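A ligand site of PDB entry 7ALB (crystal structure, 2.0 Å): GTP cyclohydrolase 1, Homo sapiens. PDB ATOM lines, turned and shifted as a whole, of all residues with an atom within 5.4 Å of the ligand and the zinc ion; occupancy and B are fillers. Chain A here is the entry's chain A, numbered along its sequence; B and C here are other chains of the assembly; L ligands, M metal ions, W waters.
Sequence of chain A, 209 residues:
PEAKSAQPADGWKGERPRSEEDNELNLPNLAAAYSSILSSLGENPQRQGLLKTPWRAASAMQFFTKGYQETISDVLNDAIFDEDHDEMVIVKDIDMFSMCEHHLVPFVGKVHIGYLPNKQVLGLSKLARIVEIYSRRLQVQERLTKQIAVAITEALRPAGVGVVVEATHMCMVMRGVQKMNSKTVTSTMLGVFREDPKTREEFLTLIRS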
ATOM      1  N   LEU A  76     -20.283  -4.051   8.955  1.00  0.00           N
ATOM      2  CA  LEU A  76     -19.535  -2.901   9.465  1.00  0.00           C
ATOM      3  C   LEU A  76     -19.793  -2.655  10.932  1.00  0.00           C
ATOM      4  O   LEU A  76     -18.878  -2.251  11.639  1.00  0.00           O
ATOM      5  CB  LEU A  76     -19.866  -1.668   8.653  1.00  0.00           C
ATOM      6  CG  LEU A  76     -18.844  -1.233   7.624  1.00  0.00           C
ATOM      7  CD1 LEU A  76     -18.437  -2.356   6.664  1.00  0.00           C
ATOM      8  CD2 LEU A  76     -19.372  -0.046   6.883  1.00  0.00           C
ATOM      9  N   ASN A  77     -21.045  -2.862  11.311  1.00  0.00           N
ATOM     10  CA  ASN A  77     -21.538  -2.712  12.675  1.00  0.00           C
ATOM     11  C   ASN A  77     -21.110  -1.425  13.350  1.00  0.00           C
ATOM     12  O   ASN A  77     -20.648  -1.476  14.478  1.00  0.00           O
ATOM     13  CB  ASN A  77     -21.083  -3.905  13.509  1.00  0.00           C
ATOM     14  CG  ASN A  77     -21.811  -4.021  14.820  1.00  0.00           C
ATOM     15  OD1 ASN A  77     -23.015  -3.839  14.888  1.00  0.00           O
ATOM     16  ND2 ASN A  77     -21.078  -4.333  15.875  1.00  0.00           N
ATOM     17  N   ALA A  79     -18.437   0.334  13.108  1.00  0.00           N
ATOM     18  CA  ALA A  79     -17.053   0.352  13.561  1.00  0.00           C
ATOM     19  C   ALA A  79     -16.252   1.295  12.693  1.00  0.00           C
ATOM     20  O   ALA A  79     -15.301   0.916  12.032  1.00  0.00           O
ATOM     21  CB  ALA A  79     -16.459  -1.049  13.541  1.00  0.00           C
ATOM     22  N   PHE A  81     -14.396   4.919  13.124  1.00  0.00           N
ATOM     23  CA  PHE A  81     -13.911   5.858  14.099  1.00  0.00           C
ATOM     24  C   PHE A  81     -13.419   7.126  13.460  1.00  0.00           C
ATOM     25  O   PHE A  81     -13.082   7.137  12.290  1.00  0.00           O
ATOM     26  CB  PHE A  81     -12.773   5.224  14.901  1.00  0.00           C
ATOM     27  CG  PHE A  81     -13.039   3.814  15.329  1.00  0.00           C
ATOM     28  CD1 PHE A  81     -13.955   3.537  16.323  1.00  0.00           C
ATOM     29  CD2 PHE A  81     -12.378   2.758  14.715  1.00  0.00           C
ATOM     30  CE1 PHE A  81     -14.205   2.237  16.697  1.00  0.00           C
ATOM     31  CE2 PHE A  81     -12.629   1.455  15.103  1.00  0.00           C
ATOM     32  CZ  PHE A  81     -13.547   1.195  16.086  1.00  0.00           C
ATOM     33  N   VAL A 121     -11.841   6.146   9.844  1.00  0.00           N
ATOM     34  CA  VAL A 121     -11.033   4.943   9.905  1.00  0.00           C
ATOM     35  C   VAL A 121     -11.864   3.712  10.204  1.00  0.00           C
ATOM     36  O   VAL A 121     -12.571   3.668  11.206  1.00  0.00           O
ATOM     37  CB  VAL A 121      -9.995   5.059  11.027  1.00  0.00           C
ATOM     38  CG1 VAL A 121      -9.074   3.859  11.019  1.00  0.00           C
ATOM     39  CG2 VAL A 121      -9.212   6.350  10.895  1.00  0.00           C
ATOM     40  N   LEU A 122     -11.765   2.702   9.354  1.00  0.00           N
ATOM     41  CA  LEU A 122     -12.510   1.474   9.554  1.00  0.00           C
ATOM     42  C   LEU A 122     -11.875   0.589  10.619  1.00  0.00           C
ATOM     43  O   LEU A 122     -10.678   0.597  10.817  1.00  0.00           O
ATOM     44  CB  LEU A 122     -12.617   0.698   8.238  1.00  0.00           C
ATOM     45  CG  LEU A 122     -13.506  -0.554   8.193  1.00  0.00           C
ATOM     46  CD1 LEU A 122     -14.835  -0.304   8.867  1.00  0.00           C
ATOM     47  CD2 LEU A 122     -13.695  -1.061   6.768  1.00  0.00           C
ATOM     48  N   GLY A 123     -12.709  -0.163  11.307  1.00  0.00           N
ATOM     49  CA  GLY A 123     -12.219  -1.090  12.297  1.00  0.00           C
ATOM     50  C   GLY A 123     -11.436  -2.164  11.583  1.00  0.00           C
ATOM     51  O   GLY A 123     -11.920  -2.720  10.618  1.00  0.00           O
ATOM     52  N   LEU A 124     -10.238  -2.462  12.064  1.00  0.00           N
ATOM     53  CA  LEU A 124      -9.351  -3.445  11.431  1.00  0.00           C
ATOM     54  C   LEU A 124      -9.994  -4.766  11.010  1.00  0.00           C
ATOM     55  O   LEU A 124      -9.829  -5.203   9.884  1.00  0.00           O
ATOM     56  CB  LEU A 124      -8.110  -3.725  12.291  1.00  0.00           C
ATOM     57  CG  LEU A 124      -7.108  -2.571  12.406  1.00  0.00           C
ATOM     58  CD1 LEU A 124      -6.026  -2.846  13.426  1.00  0.00           C
ATOM     59  CD2 LEU A 124      -6.516  -2.223  11.067  1.00  0.00           C
ATOM     60  N   SER A 125     -10.758  -5.366  11.913  1.00  0.00           N
ATOM     61  CA  SER A 125     -11.422  -6.627  11.620  1.00  0.00           C
ATOM     62  C   SER A 125     -12.478  -6.523  10.522  1.00  0.00           C
ATOM     63  O   SER A 125     -12.699  -7.470   9.798  1.00  0.00           O
ATOM     64  CB  SER A 125     -12.033  -7.223  12.881  1.00  0.00           C
ATOM     65  OG  SER A 125     -13.281  -6.646  13.184  1.00  0.00           O
ATOM     66  N   LYS A 126     -13.120  -5.368  10.381  1.00  0.00           N
ATOM     67  CA  LYS A 126     -14.127  -5.200   9.354  1.00  0.00           C
ATOM     68  C   LYS A 126     -13.565  -5.408   7.948  1.00  0.00           C
ATOM     69  O   LYS A 126     -14.270  -5.856   7.071  1.00  0.00           O
ATOM     70  CB  LYS A 126     -14.829  -3.843   9.469  1.00  0.00           C
ATOM     71  CG  LYS A 126     -15.347  -3.533  10.858  1.00  0.00           C
ATOM     72  CD  LYS A 126     -16.100  -4.706  11.448  1.00  0.00           C
ATOM     73  CE  LYS A 126     -16.456  -4.472  12.895  1.00  0.00           C
ATOM     74  NZ  LYS A 126     -17.489  -5.409  13.376  1.00  0.00           N
ATOM     75  N   ARG A 129     -13.869  -8.882   7.491  1.00  0.00           N
ATOM     76  CA  ARG A 129     -15.294  -9.228   7.421  1.00  0.00           C
ATOM     77  C   ARG A 129     -15.855  -8.914   6.035  1.00  0.00           C
ATOM     78  O   ARG A 129     -16.704  -9.640   5.541  1.00  0.00           O
ATOM     79  CB  ARG A 129     -16.116  -8.541   8.520  1.00  0.00           C
ATOM     80  CG  ARG A 129     -15.720  -8.920   9.925  1.00  0.00           C
ATOM     81  CD  ARG A 129     -16.890  -9.085  10.874  1.00  0.00           C
ATOM     82  NE  ARG A 129     -16.487  -9.461  12.230  1.00  0.00           N
ATOM     83  CZ  ARG A 129     -16.591 -10.673  12.748  1.00  0.00           C
ATOM     84  NH1 ARG A 129     -17.074 -11.651  12.018  1.00  0.00           N
ATOM     85  NH2 ARG A 129     -16.209 -10.912  13.986  1.00  0.00           N
ATOM     86  N   CYS B 100      -4.811  -3.863  22.851  1.00  0.00           N
ATOM     87  CA  CYS B 100      -5.901  -3.273  22.140  1.00  0.00           C
ATOM     88  C   CYS B 100      -6.882  -2.621  23.106  1.00  0.00           C
ATOM     89  O   CYS B 100      -7.364  -3.256  24.037  1.00  0.00           O
ATOM     90  CB  CYS B 100      -6.610  -4.339  21.318  1.00  0.00           C
ATOM     91  SG  CYS B 100      -8.204  -3.827  20.698  1.00  0.00           S
ATOM     92  N   HIS B 102      -9.927  -1.694  22.506  1.00  0.00           N
ATOM     93  CA  HIS B 102     -11.291  -2.142  22.311  1.00  0.00           C
ATOM     94  C   HIS B 102     -11.630  -3.498  22.940  1.00  0.00           C
ATOM     95  O   HIS B 102     -12.757  -3.724  23.342  1.00  0.00           O
ATOM     96  CB  HIS B 102     -11.647  -2.101  20.828  1.00  0.00           C
ATOM     97  CG  HIS B 102     -11.486  -0.745  20.210  1.00  0.00           C
ATOM     98  ND1 HIS B 102     -12.206   0.345  20.614  1.00  0.00           N
ATOM     99  CD2 HIS B 102     -10.665  -0.315  19.225  1.00  0.00           C
ATOM    100  CE1 HIS B 102     -11.852   1.389  19.897  1.00  0.00           C
ATOM    101  NE2 HIS B 102     -10.917   1.019  19.054  1.00  0.00           N
ATOM    102  N   HIS B 103     -10.645  -4.387  23.044  1.00  0.00           N
ATOM    103  CA  HIS B 103     -10.897  -5.708  23.602  1.00  0.00           C
ATOM    104  C   HIS B 103     -10.033  -6.097  24.792  1.00  0.00           C
ATOM    105  O   HIS B 103     -10.308  -7.135  25.381  1.00  0.00           O
ATOM    106  CB  HIS B 103     -10.699  -6.784  22.529  1.00  0.00           C
ATOM    107  CG  HIS B 103     -11.703  -6.778  21.423  1.00  0.00           C
ATOM    108  ND1 HIS B 103     -11.484  -6.131  20.226  1.00  0.00           N
ATOM    109  CD2 HIS B 103     -12.900  -7.386  21.304  1.00  0.00           C
ATOM    110  CE1 HIS B 103     -12.514  -6.317  19.432  1.00  0.00           C
ATOM    111  NE2 HIS B 103     -13.389  -7.076  20.063  1.00  0.00           N
ATOM    112  N   VAL B 105      -6.891  -7.106  24.714  1.00  0.00           N
ATOM    113  CA  VAL B 105      -6.179  -8.280  24.276  1.00  0.00           C
ATOM    114  C   VAL B 105      -4.906  -7.788  23.562  1.00  0.00           C
ATOM    115  O   VAL B 105      -4.951  -6.744  22.891  1.00  0.00           O
ATOM    116  CB  VAL B 105      -7.117  -9.113  23.350  1.00  0.00           C
ATOM    117  CG1 VAL B 105      -6.369 -10.247  22.677  1.00  0.00           C
ATOM    118  CG2 VAL B 105      -8.325  -9.659  24.117  1.00  0.00           C
ATOM    119  N   PHE B 107      -1.718  -6.941  21.072  1.00  0.00           N
ATOM    120  CA  PHE B 107      -1.341  -6.862  19.673  1.00  0.00           C
ATOM    121  C   PHE B 107       0.187  -6.682  19.696  1.00  0.00           C
ATOM    122  O   PHE B 107       0.711  -5.898  20.489  1.00  0.00           O
ATOM    123  CB  PHE B 107      -2.115  -5.851  18.818  1.00  0.00           C
ATOM    124  CG  PHE B 107      -1.884  -4.380  19.025  1.00  0.00           C
ATOM    125  CD1 PHE B 107      -0.993  -3.681  18.230  1.00  0.00           C
ATOM    126  CD2 PHE B 107      -2.691  -3.652  19.894  1.00  0.00           C
ATOM    127  CE1 PHE B 107      -0.853  -2.303  18.349  1.00  0.00           C
ATOM    128  CE2 PHE B 107      -2.552  -2.266  20.007  1.00  0.00           C
ATOM    129  CZ  PHE B 107      -1.653  -1.603  19.212  1.00  0.00           C
ATOM    130  N   GLN B 139      -4.220   0.917  23.368  1.00  0.00           N
ATOM    131  CA  GLN B 139      -4.044   1.574  22.104  1.00  0.00           C
ATOM    132  C   GLN B 139      -4.805   1.080  20.899  1.00  0.00           C
ATOM    133  O   GLN B 139      -5.550   0.119  20.940  1.00  0.00           O
ATOM    134  CB  GLN B 139      -2.571   1.413  21.719  1.00  0.00           C
ATOM    135  CG  GLN B 139      -1.619   2.366  22.389  1.00  0.00           C
ATOM    136  CD  GLN B 139      -1.580   3.705  21.711  1.00  0.00           C
ATOM    137  OE1 GLN B 139      -2.419   4.006  20.890  1.00  0.00           O
ATOM    138  NE2 GLN B 139      -0.612   4.511  22.053  1.00  0.00           N
ATOM    139  N   VAL B 140      -4.569   1.802  19.830  1.00  0.00           N
ATOM    140  CA  VAL B 140      -5.042   1.506  18.494  1.00  0.00           C
ATOM    141  C   VAL B 140      -3.765   1.717  17.668  1.00  0.00           C
ATOM    142  O   VAL B 140      -3.036   2.668  17.886  1.00  0.00           O
ATOM    143  CB  VAL B 140      -6.223   2.359  18.028  1.00  0.00           C
ATOM    144  CG1 VAL B 140      -7.511   1.884  18.678  1.00  0.00           C
ATOM    145  CG2 VAL B 140      -5.980   3.839  18.282  1.00  0.00           C
ATOM    146  N   GLN B 141      -3.492   0.805  16.755  1.00  0.00           N
ATOM    147  CA  GLN B 141      -2.269   0.858  15.955  1.00  0.00           C
ATOM    148  C   GLN B 141      -1.988   2.205  15.303  1.00  0.00           C
ATOM    149  O   GLN B 141      -0.905   2.719  15.426  1.00  0.00           O
ATOM    150  CB  GLN B 141      -2.234  -0.257  14.922  1.00  0.00           C
ATOM    151  CG  GLN B 141      -0.852  -0.491  14.351  1.00  0.00           C
ATOM    152  CD  GLN B 141      -0.683  -1.875  13.760  1.00  0.00           C
ATOM    153  OE1 GLN B 141      -1.288  -2.817  14.219  1.00  0.00           O
ATOM    154  NE2 GLN B 141       0.140  -1.977  12.739  1.00  0.00           N
ATOM    155  N   GLU B 142      -2.988   2.769  14.647  1.00  0.00           N
ATOM    156  CA  GLU B 142      -2.856   4.053  13.981  1.00  0.00           C
ATOM    157  C   GLU B 142      -2.344   5.158  14.894  1.00  0.00           C
ATOM    158  O   GLU B 142      -1.449   5.886  14.520  1.00  0.00           O
ATOM    159  CB  GLU B 142      -4.172   4.478  13.349  1.00  0.00           C
ATOM    160  CG  GLU B 142      -4.562   3.634  12.156  1.00  0.00           C
ATOM    161  CD  GLU B 142      -5.446   2.481  12.562  1.00  0.00           C
ATOM    162  OE1 GLU B 142      -6.307   2.075  11.773  1.00  0.00           O
ATOM    163  OE2 GLU B 142      -5.302   1.979  13.682  1.00  0.00           O
ATOM    164  N   HIS B 169      -2.765  -8.832  15.553  1.00  0.00           N
ATOM    165  CA  HIS B 169      -3.722  -8.522  16.562  1.00  0.00           C
ATOM    166  C   HIS B 169      -4.348  -9.840  16.988  1.00  0.00           C
ATOM    167  O   HIS B 169      -5.005 -10.487  16.204  1.00  0.00           O
ATOM    168  CB  HIS B 169      -4.761  -7.552  16.012  1.00  0.00           C
ATOM    169  CG  HIS B 169      -4.246  -6.153  15.869  1.00  0.00           C
ATOM    170  ND1 HIS B 169      -4.691  -5.105  16.634  1.00  0.00           N
ATOM    171  CD2 HIS B 169      -3.283  -5.643  15.069  1.00  0.00           C
ATOM    172  CE1 HIS B 169      -4.045  -4.009  16.308  1.00  0.00           C
ATOM    173  NE2 HIS B 169      -3.180  -4.306  15.350  1.00  0.00           N
ATOM    174  N   CYS B 171      -6.972 -10.293  18.749  1.00  0.00           N
ATOM    175  CA  CYS B 171      -8.404 -10.154  18.537  1.00  0.00           C
ATOM    176  C   CYS B 171      -8.859 -10.589  17.136  1.00  0.00           C
ATOM    177  O   CYS B 171     -10.033 -10.878  16.966  1.00  0.00           O
ATOM    178  CB  CYS B 171      -8.816  -8.705  18.797  1.00  0.00           C
ATOM    179  SG  CYS B 171      -8.217  -8.092  20.368  1.00  0.00           S
ATOM    180  N   MET B 172      -7.965 -10.597  16.136  1.00  0.00           N
ATOM    181  CA  MET B 172      -8.295 -11.091  14.808  1.00  0.00           C
ATOM    182  C   MET B 172      -7.837 -12.525  14.564  1.00  0.00           C
ATOM    183  O   MET B 172      -8.166 -13.072  13.515  1.00  0.00           O
ATOM    184  CB  MET B 172      -7.740 -10.158  13.731  1.00  0.00           C
ATOM    185  CG  MET B 172      -8.370  -8.759  13.790  1.00  0.00           C
ATOM    186  SD  MET B 172      -7.834  -7.688  12.435  1.00  0.00           S
ATOM    187  CE  MET B 172      -6.060  -7.623  12.698  1.00  0.00           C
ATOM    188  N   ARG B 175      -9.989 -15.012  18.010  1.00  0.00           N
ATOM    189  CA  ARG B 175     -11.422 -14.764  18.069  1.00  0.00           C
ATOM    190  C   ARG B 175     -11.870 -13.912  16.906  1.00  0.00           C
ATOM    191  O   ARG B 175     -11.087 -13.580  16.034  1.00  0.00           O
ATOM    192  CB  ARG B 175     -11.750 -14.002  19.344  1.00  0.00           C
ATOM    193  CG  ARG B 175     -10.978 -12.700  19.482  1.00  0.00           C
ATOM    194  CD  ARG B 175     -11.616 -11.696  20.429  1.00  0.00           C
ATOM    195  NE  ARG B 175     -12.990 -11.391  20.077  1.00  0.00           N
ATOM    196  CZ  ARG B 175     -13.365 -10.605  19.075  1.00  0.00           C
ATOM    197  NH1 ARG B 175     -12.467 -10.016  18.315  1.00  0.00           N
ATOM    198  NH2 ARG B 175     -14.644 -10.407  18.856  1.00  0.00           N
ATOM    199  N   GLY B 176     -13.137 -13.542  16.922  1.00  0.00           N
ATOM    200  CA  GLY B 176     -13.728 -12.733  15.881  1.00  0.00           C
ATOM    201  C   GLY B 176     -13.595 -13.392  14.521  1.00  0.00           C
ATOM    202  O   GLY B 176     -14.035 -14.507  14.319  1.00  0.00           O
ATOM    203  N   VAL B 177     -12.975 -12.680  13.592  1.00  0.00           N
ATOM    204  CA  VAL B 177     -12.766 -13.167  12.241  1.00  0.00           C
ATOM    205  C   VAL B 177     -11.892 -14.386  12.159  1.00  0.00           C
ATOM    206  O   VAL B 177     -11.987 -15.114  11.183  1.00  0.00           O
ATOM    207  CB  VAL B 177     -12.248 -12.077  11.260  1.00  0.00           C
ATOM    208  CG1 VAL B 177     -13.315 -11.062  10.978  1.00  0.00           C
ATOM    209  CG2 VAL B 177     -10.967 -11.417  11.784  1.00  0.00           C
ATOM    210  N   LYS C  52     -17.297   0.927  24.741  1.00  0.00           N
ATOM    211  CA  LYS C  52     -17.738  -0.436  24.477  1.00  0.00           C
ATOM    212  C   LYS C  52     -16.801  -1.532  24.982  1.00  0.00           C
ATOM    213  O   LYS C  52     -17.156  -2.693  24.968  1.00  0.00           O
ATOM    214  CB  LYS C  52     -17.984  -0.619  22.986  1.00  0.00           C
ATOM    215  CG  LYS C  52     -19.353  -0.158  22.524  1.00  0.00           C
ATOM    216  CD  LYS C  52     -19.477  -0.219  21.013  1.00  0.00           C
ATOM    217  CE  LYS C  52     -20.285   0.963  20.490  1.00  0.00           C
ATOM    218  NZ  LYS C  52     -20.808   0.682  19.130  1.00  0.00           N
ATOM    219  N   ARG C  56     -16.963  -5.681  25.280  1.00  0.00           N
ATOM    220  CA  ARG C  56     -16.156  -6.389  24.314  1.00  0.00           C
ATOM    221  C   ARG C  56     -15.114  -7.273  24.992  1.00  0.00           C
ATOM    222  O   ARG C  56     -14.913  -8.396  24.586  1.00  0.00           O
ATOM    223  CB  ARG C  56     -15.526  -5.424  23.310  1.00  0.00           C
ATOM    224  CG  ARG C  56     -16.544  -4.847  22.334  1.00  0.00           C
ATOM    225  CD  ARG C  56     -15.887  -4.181  21.151  1.00  0.00           C
ATOM    226  NE  ARG C  56     -15.339  -2.889  21.490  1.00  0.00           N
ATOM    227  CZ  ARG C  56     -15.611  -1.764  20.849  1.00  0.00           C
ATOM    228  NH1 ARG C  56     -16.450  -1.774  19.837  1.00  0.00           N
ATOM    229  NH2 ARG C  56     -15.079  -0.634  21.239  1.00  0.00           N
HETATM  230  O1  LIG L   1     -18.017  -4.433  16.045  1.00  0.00           O
HETATM  231  C1  LIG L   1      -9.481  -2.930  17.415  1.00  0.00           C
HETATM  232  C2  LIG L   1     -11.420  -2.718  15.792  1.00  0.00           C
HETATM  233  O2  LIG L   1     -16.515  -5.128  17.954  1.00  0.00           O
HETATM  234  C3  LIG L   1     -13.653  -2.724  16.033  1.00  0.00           C
HETATM  235  N1  LIG L   1      -9.562  -0.764  14.658  1.00  0.00           N
HETATM  236  C4  LIG L   1     -14.698  -2.789  17.111  1.00  0.00           C
HETATM  237  C5  LIG L   1     -13.260  -4.070  15.408  1.00  0.00           C
HETATM  238  N2  LIG L   1     -10.120  -2.360  16.332  1.00  0.00           N
HETATM  239  C6  LIG L   1     -11.768  -4.190  15.747  1.00  0.00           C
HETATM  240  O3  LIG L   1     -15.753  -7.240  18.903  1.00  0.00           O
HETATM  241  C7  LIG L   1      -6.987  -0.737  15.904  1.00  0.00           C
HETATM  242  O4  LIG L   1     -17.762  -7.265  17.460  1.00  0.00           O
HETATM  243  N3  LIG L   1      -7.340   0.039  14.830  1.00  0.00           N
HETATM  244  O5  LIG L   1     -15.502  -6.866  16.486  1.00  0.00           O
HETATM  245  O6  LIG L   1     -15.623  -9.321  16.220  1.00  0.00           O
HETATM  246  N4  LIG L   1      -8.802   0.859  13.243  1.00  0.00           N
HETATM  247  C8  LIG L   1      -8.581   0.021  14.247  1.00  0.00           C
HETATM  248  O7  LIG L   1     -12.438  -2.138  16.548  1.00  0.00           O
HETATM  249  C9  LIG L   1      -9.256  -1.513  15.726  1.00  0.00           C
HETATM  250  C10 LIG L   1      -8.047  -1.558  16.401  1.00  0.00           C
HETATM  251  C11 LIG L   1      -8.204  -2.461  17.475  1.00  0.00           C
HETATM  252  O8  LIG L   1     -15.900  -3.253  16.471  1.00  0.00           O
HETATM  253  O9  LIG L   1     -15.021  -7.961  14.368  1.00  0.00           O
HETATM  254  O10 LIG L   1     -13.460  -4.036  13.998  1.00  0.00           O
HETATM  255  O11 LIG L   1     -10.993  -4.817  14.744  1.00  0.00           O
HETATM  256  O12 LIG L   1      -5.833  -0.730  16.323  1.00  0.00           O
HETATM  257  O13 LIG L   1     -17.758  -3.017  18.018  1.00  0.00           O
HETATM  258  O14 LIG L   1     -13.515  -8.164  16.182  1.00  0.00           O
HETATM  259  P1  LIG L   1     -17.124  -3.956  17.078  1.00  0.00           P
HETATM  260  P2  LIG L   1     -16.466  -6.703  17.746  1.00  0.00           P
HETATM  261  P3  LIG L   1     -14.921  -8.169  15.788  1.00  0.00           P
HETATM  262 ZN    ZN M   1      -9.261  -5.883  19.717  1.00  0.00          ZN
HETATM  263  O   HOH W   1     -11.716 -10.033  14.751  1.00  0.00           O
HETATM  264  O   HOH W   2     -10.904  -7.266  16.037  1.00  0.00           O
HETATM  265  O   HOH W   3     -18.864  -7.756  15.217  1.00  0.00           O
HETATM  266  O   HOH W   4      -7.952  -5.757  17.195  1.00  0.00           O
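The backbone NH of Ser 125 lies within hydrogen-bond range of the side-chain sulfur of Met 172 of chain B (3.8 Å).
The side-chain sulfur of Cys 100 of chain B lies close to the backbone NH of His 102 of chain B (3.3 Å).
NH1 of Arg 175 of chain B lies within hydrogen-bond range of O of Cys 171 of chain B, 2.9 Å away.
ND1 of His 102 of chain B lies within hydrogen-bond range of NH2 of Arg 56 of chain C, 3.1 Å away.
A ring nitrogen (NE2) of His 169 of chain B is in hydrogen-bond range of the side-chain amide oxygen of Gln 141 of chain B (2.7 Å).
The backbone carbonyl oxygen (O) of Phe 81 lies within hydrogen-bond range of the backbone NH (N) of Val 121.
O of Ala 79 is in hydrogen-bond range of N of Gly 123, 2.9 Å away.
A ring nitrogen (NE2) of His 103 of chain B is in hydrogen-bond range of an oxygen (O3) of the ligand (2.6 Å).
The backbone NH (N) of Ser 125 sits at hydrogen-bond distance from an oxygen (O11) of the ligand, at 2.9 Å.
The side-chain hydroxyl (OG) of Ser 125 is in hydrogen-bond range of an oxygen (O9) of the ligand (2.5 Å).
NH1 of Arg 56 of chain C lies within salt-bridge range of O13 of the ligand, 2.6 Å away.
The guanidinium group (NH2) of Arg 129 is in salt-bridge range of an oxygen (O6) of the ligand (2.8 Å).
N of Gln 141 of chain B sits at hydrogen-bond distance from O12 of the ligand (2.8 Å).
NZ of Lys 126 lies within salt-bridge range of O1 of the ligand, 2.9 Å away.
NH1 of Arg 175 of chain B lies within salt-bridge range of O14 of the ligand (3.0 Å).
The side-chain carboxylate (OE2) of Glu 142 of chain B sits at hydrogen-bond distance from a nitrogen (N3) of the ligand (3.0 Å).
The side-chain amide nitrogen (ND2) of Asn 77 lies within hydrogen-bond range of an oxygen (O1) of the ligand (3.1 Å).
N4 of the ligand lies within hydrogen-bond range of O of Leu 122, 3.1 Å away.
N of Leu 124 sits at hydrogen-bond distance from N1 of the ligand (3.2 Å).
Water W3 bridges an oxygen (O4) of the ligand (2.5 Å) and the side-chain amino group (NZ) of Lys 126 (3.3 Å).
Water W1 lies within hydrogen-bond range of O of Cys 171 of chain B, O14 of the ligand and N of Val 177 of chain B.
A ring nitrogen (ND1) of His 103 of chain B binds the zinc ion (2.3 Å).
SG of Cys 100 of chain B binds the zinc ion (2.5 Å).
The zinc ion is bound by SG of Cys 171 of chain B, at 2.5 Å.
Slightly farther from the zinc ion lies water W4 (2.8 Å).
Merely in contact with the ligand: Ala 79, Phe 81, Val 121, Gly 123, His 102 of chain B, Val 140 of chain B, His 169 of chain B and Gly 176 of chain B.
Hydrophobic or aromatic side chains within 4 Å of the ligand: Ala 79, Phe 81, Val 121, Leu 124, His 102 of chain B, His 103 of chain B, Val 140 of chain B and His 169 of chain B.
Of the 28 residues printed, 20 come within 4 Å of the ligand.
The nearest printed residue that does not touch the zinc ion is His 102 of chain B (4.6 Å).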
